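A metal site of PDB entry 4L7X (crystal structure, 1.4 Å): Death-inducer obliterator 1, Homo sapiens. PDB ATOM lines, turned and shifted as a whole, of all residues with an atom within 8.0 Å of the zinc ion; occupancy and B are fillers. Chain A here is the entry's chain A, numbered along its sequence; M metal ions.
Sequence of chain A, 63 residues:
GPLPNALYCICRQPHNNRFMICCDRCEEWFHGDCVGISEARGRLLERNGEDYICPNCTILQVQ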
ATOM      1  N   TYR A   8      -8.476  -2.365 -18.027  1.00  0.00           N
ATOM      2  CA  TYR A   8      -8.264  -2.406 -16.585  1.00  0.00           C
ATOM      3  C   TYR A   8      -8.795  -1.155 -15.907  1.00  0.00           C
ATOM      4  O   TYR A   8      -9.209  -0.192 -16.569  1.00  0.00           O
ATOM      5  CB  TYR A   8      -6.768  -2.522 -16.281  1.00  0.00           C
ATOM      6  CG  TYR A   8      -6.129  -3.739 -16.895  1.00  0.00           C
ATOM      7  CD1 TYR A   8      -5.369  -3.635 -18.043  1.00  0.00           C
ATOM      8  CD2 TYR A   8      -6.325  -4.988 -16.342  1.00  0.00           C
ATOM      9  CE1 TYR A   8      -4.802  -4.748 -18.623  1.00  0.00           C
ATOM     10  CE2 TYR A   8      -5.754  -6.104 -16.909  1.00  0.00           C
ATOM     11  CZ  TYR A   8      -4.995  -5.989 -18.039  1.00  0.00           C
ATOM     12  OH  TYR A   8      -4.441  -7.117 -18.588  1.00  0.00           O
ATOM     13  N   CYS A   9      -8.765  -1.172 -14.583  1.00  0.00           N
ATOM     14  CA  CYS A   9      -8.848   0.030 -13.768  1.00  0.00           C
ATOM     15  C   CYS A   9     -10.246   0.669 -13.727  1.00  0.00           C
ATOM     16  O   CYS A   9     -11.208   0.147 -14.295  1.00  0.00           O
ATOM     17  CB  CYS A   9      -7.781   1.033 -14.252  1.00  0.00           C
ATOM     18  SG  CYS A   9      -7.410   2.464 -13.190  1.00  0.00           S
ATOM     19  N   ILE A  10     -10.349   1.770 -12.992  1.00  0.00           N
ATOM     20  CA  ILE A  10     -11.596   2.536 -12.947  1.00  0.00           C
ATOM     21  C   ILE A  10     -11.856   3.157 -14.310  1.00  0.00           C
ATOM     22  O   ILE A  10     -13.017   3.335 -14.719  1.00  0.00           O
ATOM     23  CB  ILE A  10     -11.500   3.650 -11.878  1.00  0.00           C
ATOM     24  CG1 ILE A  10     -11.462   3.048 -10.475  1.00  0.00           C
ATOM     25  CG2 ILE A  10     -12.691   4.594 -11.986  1.00  0.00           C
ATOM     26  CD1 ILE A  10     -11.046   4.029  -9.407  1.00  0.00           C
ATOM     27  N   CYS A  11     -10.778   3.470 -15.016  1.00  0.00           N
ATOM     28  CA  CYS A  11     -10.857   4.197 -16.284  1.00  0.00           C
ATOM     29  C   CYS A  11     -11.194   3.302 -17.480  1.00  0.00           C
ATOM     30  O   CYS A  11     -11.534   3.808 -18.560  1.00  0.00           O
ATOM     31  CB  CYS A  11      -9.535   4.925 -16.544  1.00  0.00           C
ATOM     32  SG  CYS A  11      -8.116   3.829 -16.748  1.00  0.00           S
ATOM     33  N   ARG A  12     -11.093   1.988 -17.310  1.00  0.00           N
ATOM     34  CA  ARG A  12     -11.385   1.050 -18.394  1.00  0.00           C
ATOM     35  C   ARG A  12     -10.506   1.315 -19.612  1.00  0.00           C
ATOM     36  O   ARG A  12     -11.002   1.473 -20.754  1.00  0.00           O
ATOM     37  CB  ARG A  12     -12.875   1.079 -18.775  1.00  0.00           C
ATOM     38  CG  ARG A  12     -13.844   0.943 -17.611  1.00  0.00           C
ATOM     39  CD  ARG A  12     -13.421  -0.122 -16.617  1.00  0.00           C
ATOM     40  NE  ARG A  12     -13.394  -1.459 -17.215  1.00  0.00           N
ATOM     41  CZ  ARG A  12     -12.669  -2.470 -16.768  1.00  0.00           C
ATOM     42  NH1 ARG A  12     -11.872  -2.331 -15.702  1.00  0.00           N
ATOM     43  NH2 ARG A  12     -12.743  -3.642 -17.385  1.00  0.00           N
ATOM     44  N   GLN A  13      -9.196   1.357 -19.368  1.00  0.00           N
ATOM     45  CA  GLN A  13      -8.200   1.541 -20.407  1.00  0.00           C
ATOM     46  C   GLN A  13      -7.128   0.473 -20.335  1.00  0.00           C
ATOM     47  O   GLN A  13      -6.999  -0.196 -19.308  1.00  0.00           O
ATOM     48  CB  GLN A  13      -7.553   2.911 -20.264  1.00  0.00           C
ATOM     49  CG  GLN A  13      -8.544   4.081 -20.331  1.00  0.00           C
ATOM     50  NE2 GLN A  13      -8.287   4.245 -22.749  1.00  0.00           N
ATOM     51  N   PRO A  14      -6.360   0.297 -21.415  1.00  0.00           N
ATOM     52  CA  PRO A  14      -5.290  -0.709 -21.412  1.00  0.00           C
ATOM     53  C   PRO A  14      -4.147  -0.374 -20.468  1.00  0.00           C
ATOM     54  O   PRO A  14      -4.059   0.729 -19.918  1.00  0.00           O
ATOM     55  CB  PRO A  14      -4.793  -0.702 -22.870  1.00  0.00           C
ATOM     56  CG  PRO A  14      -5.969  -0.150 -23.674  1.00  0.00           C
ATOM     57  CD  PRO A  14      -6.548   0.893 -22.747  1.00  0.00           C
ATOM     58  N   ARG A  18       2.160   1.396 -18.462  1.00  0.00           N
ATOM     59  CA  ARG A  18       2.023   2.300 -17.334  1.00  0.00           C
ATOM     60  C   ARG A  18       2.231   1.553 -16.030  1.00  0.00           C
ATOM     61  O   ARG A  18       1.984   0.333 -15.935  1.00  0.00           O
ATOM     62  CB  ARG A  18       0.630   2.944 -17.339  1.00  0.00           C
ATOM     63  CG  ARG A  18       0.377   3.831 -18.555  1.00  0.00           C
ATOM     64  CD  ARG A  18      -1.089   4.197 -18.702  1.00  0.00           C
ATOM     65  NE  ARG A  18      -1.607   5.036 -17.615  1.00  0.00           N
ATOM     66  CZ  ARG A  18      -2.881   5.411 -17.526  1.00  0.00           C
ATOM     67  NH1 ARG A  18      -3.754   5.027 -18.451  1.00  0.00           N
ATOM     68  NH2 ARG A  18      -3.282   6.177 -16.519  1.00  0.00           N
ATOM     69  N   PHE A  19       2.642   2.289 -15.004  1.00  0.00           N
ATOM     70  CA  PHE A  19       2.761   1.719 -13.667  1.00  0.00           C
ATOM     71  C   PHE A  19       1.364   1.326 -13.171  1.00  0.00           C
ATOM     72  O   PHE A  19       0.438   2.147 -13.206  1.00  0.00           O
ATOM     73  CB  PHE A  19       3.401   2.722 -12.684  1.00  0.00           C
ATOM     74  CG  PHE A  19       3.166   2.391 -11.239  1.00  0.00           C
ATOM     75  CD1 PHE A  19       3.573   1.171 -10.728  1.00  0.00           C
ATOM     76  CD2 PHE A  19       2.459   3.249 -10.420  1.00  0.00           C
ATOM     77  CE1 PHE A  19       3.313   0.851  -9.410  1.00  0.00           C
ATOM     78  CE2 PHE A  19       2.204   2.921  -9.113  1.00  0.00           C
ATOM     79  CZ  PHE A  19       2.620   1.715  -8.618  1.00  0.00           C
ATOM     80  N   MET A  20       1.220   0.080 -12.741  1.00  0.00           N
ATOM     81  CA  MET A  20      -0.051  -0.409 -12.234  1.00  0.00           C
ATOM     82  C   MET A  20       0.135  -1.232 -10.972  1.00  0.00           C
ATOM     83  O   MET A  20       1.217  -1.761 -10.705  1.00  0.00           O
ATOM     84  CB  MET A  20      -0.782  -1.284 -13.270  1.00  0.00           C
ATOM     85  CG  MET A  20      -1.024  -0.583 -14.604  1.00  0.00           C
ATOM     86  SD  MET A  20      -2.100  -1.489 -15.723  1.00  0.00           S
ATOM     87  CE  MET A  20      -3.678  -1.219 -14.946  1.00  0.00           C
ATOM     88  N   TRP A  29      -6.732  -4.594 -11.728  1.00  0.00           N
ATOM     89  CA  TRP A  29      -5.514  -3.807 -11.839  1.00  0.00           C
ATOM     90  C   TRP A  29      -5.832  -2.334 -12.067  1.00  0.00           C
ATOM     91  O   TRP A  29      -6.765  -2.006 -12.822  1.00  0.00           O
ATOM     92  CB  TRP A  29      -4.648  -4.312 -12.986  1.00  0.00           C
ATOM     93  CG  TRP A  29      -3.951  -5.594 -12.710  1.00  0.00           C
ATOM     94  CD1 TRP A  29      -4.427  -6.856 -12.899  1.00  0.00           C
ATOM     95  CD2 TRP A  29      -2.624  -5.733 -12.178  1.00  0.00           C
ATOM     96  NE1 TRP A  29      -3.490  -7.775 -12.525  1.00  0.00           N
ATOM     97  CE2 TRP A  29      -2.370  -7.116 -12.083  1.00  0.00           C
ATOM     98  CE3 TRP A  29      -1.636  -4.836 -11.789  1.00  0.00           C
ATOM     99  CZ2 TRP A  29      -1.159  -7.613 -11.615  1.00  0.00           C
ATOM    100  CZ3 TRP A  29      -0.434  -5.340 -11.311  1.00  0.00           C
ATOM    101  CH2 TRP A  29      -0.208  -6.704 -11.241  1.00  0.00           C
ATOM    102  N   PHE A  30      -5.039  -1.475 -11.453  1.00  0.00           N
ATOM    103  CA  PHE A  30      -5.266  -0.031 -11.457  1.00  0.00           C
ATOM    104  C   PHE A  30      -3.991   0.703 -11.869  1.00  0.00           C
ATOM    105  O   PHE A  30      -2.909   0.376 -11.408  1.00  0.00           O
ATOM    106  CB  PHE A  30      -5.731   0.431 -10.074  1.00  0.00           C
ATOM    107  CG  PHE A  30      -7.039  -0.171  -9.680  1.00  0.00           C
ATOM    108  CD1 PHE A  30      -7.072  -1.399  -9.032  1.00  0.00           C
ATOM    109  CD2 PHE A  30      -8.232   0.448 -10.003  1.00  0.00           C
ATOM    110  CE1 PHE A  30      -8.291  -1.981  -8.702  1.00  0.00           C
ATOM    111  CE2 PHE A  30      -9.446  -0.141  -9.685  1.00  0.00           C
ATOM    112  CZ  PHE A  30      -9.462  -1.352  -9.030  1.00  0.00           C
ATOM    113  N   HIS A  31      -4.140   1.707 -12.717  1.00  0.00           N
ATOM    114  CA  HIS A  31      -3.018   2.589 -12.988  1.00  0.00           C
ATOM    115  C   HIS A  31      -2.736   3.399 -11.717  1.00  0.00           C
ATOM    116  O   HIS A  31      -3.648   3.952 -11.110  1.00  0.00           O
ATOM    117  CB  HIS A  31      -3.334   3.549 -14.128  1.00  0.00           C
ATOM    118  CG  HIS A  31      -3.765   2.867 -15.379  1.00  0.00           C
ATOM    119  ND1 HIS A  31      -5.090   2.830 -15.777  1.00  0.00           N
ATOM    120  CD2 HIS A  31      -3.077   2.164 -16.306  1.00  0.00           C
ATOM    121  CE1 HIS A  31      -5.179   2.145 -16.907  1.00  0.00           C
ATOM    122  NE2 HIS A  31      -3.966   1.744 -17.249  1.00  0.00           N
ATOM    123  N   GLY A  32      -1.470   3.451 -11.311  1.00  0.00           N
ATOM    124  CA  GLY A  32      -1.113   4.208 -10.124  1.00  0.00           C
ATOM    125  C   GLY A  32      -1.648   5.634 -10.122  1.00  0.00           C
ATOM    126  O   GLY A  32      -2.117   6.120  -9.098  1.00  0.00           O
ATOM    127  N   ASP A  33      -1.566   6.311 -11.256  1.00  0.00           N
ATOM    128  CA  ASP A  33      -1.982   7.718 -11.306  1.00  0.00           C
ATOM    129  C   ASP A  33      -3.510   7.915 -11.289  1.00  0.00           C
ATOM    130  O   ASP A  33      -3.999   8.978 -10.930  1.00  0.00           O
ATOM    131  CB  ASP A  33      -1.281   8.483 -12.451  1.00  0.00           C
ATOM    132  CG  ASP A  33      -1.494   7.877 -13.833  1.00  0.00           C
ATOM    133  OD1 ASP A  33      -2.163   6.847 -13.972  1.00  0.00           O
ATOM    134  OD2 ASP A  33      -0.972   8.474 -14.805  1.00  0.00           O
ATOM    135  N   CYS A  34      -4.246   6.872 -11.622  1.00  0.00           N
ATOM    136  CA  CYS A  34      -5.696   6.865 -11.428  1.00  0.00           C
ATOM    137  C   CYS A  34      -6.143   6.748  -9.976  1.00  0.00           C
ATOM    138  O   CYS A  34      -7.181   7.309  -9.585  1.00  0.00           O
ATOM    139  CB  CYS A  34      -6.311   5.721 -12.209  1.00  0.00           C
ATOM    140  SG  CYS A  34      -6.258   5.983 -14.000  1.00  0.00           S
ATOM    141  N   VAL A  35      -5.384   6.022  -9.158  1.00  0.00           N
ATOM    142  CA  VAL A  35      -5.821   5.723  -7.798  1.00  0.00           C
ATOM    143  C   VAL A  35      -4.997   6.381  -6.677  1.00  0.00           C
ATOM    144  O   VAL A  35      -5.363   6.274  -5.501  1.00  0.00           O
ATOM    145  CB  VAL A  35      -5.895   4.200  -7.536  1.00  0.00           C
ATOM    146  CG1 VAL A  35      -6.941   3.587  -8.434  1.00  0.00           C
ATOM    147  CG2 VAL A  35      -4.556   3.535  -7.739  1.00  0.00           C
HETATM  148 ZN    ZN M   1      -6.750   3.911 -14.861  1.00  0.00          ZN
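The backbone NH (N) of Gln 13 lies close to the side-chain sulfur (SG) of Cys 11, 3.8 Å away. The backbone carbonyl oxygen (O) of Trp 29 is in hydrogen-bond range of the backbone NH (N) of Cys 9, at 2.8 Å. NE2 of His 31 sits at hydrogen-bond distance from O of Pro 14, at 2.9 Å. The backbone carbonyl oxygen (O) of Cys 9 sits at hydrogen-bond distance from the guanidinium group (NH1) of Arg 12 (2.9 Å).
Four residues have an atom within 4 Å of the zinc ion: Cys 9, Cys 11, His 31 and Cys 34. Along chain A the residues within 4 Å of the zinc ion span positions 9 to 34. The nearest printed residue that does not touch the zinc ion is Arg 18 (4.5 Å).
The zinc ion is bound by a ring nitrogen (ND1) of His 31, the side-chain sulfur (SG) of Cys 34, the side-chain sulfur (SG) of Cys 9 and the side-chain sulfur (SG) of Cys 11. The zinc ion has four donor atoms within binding distance.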
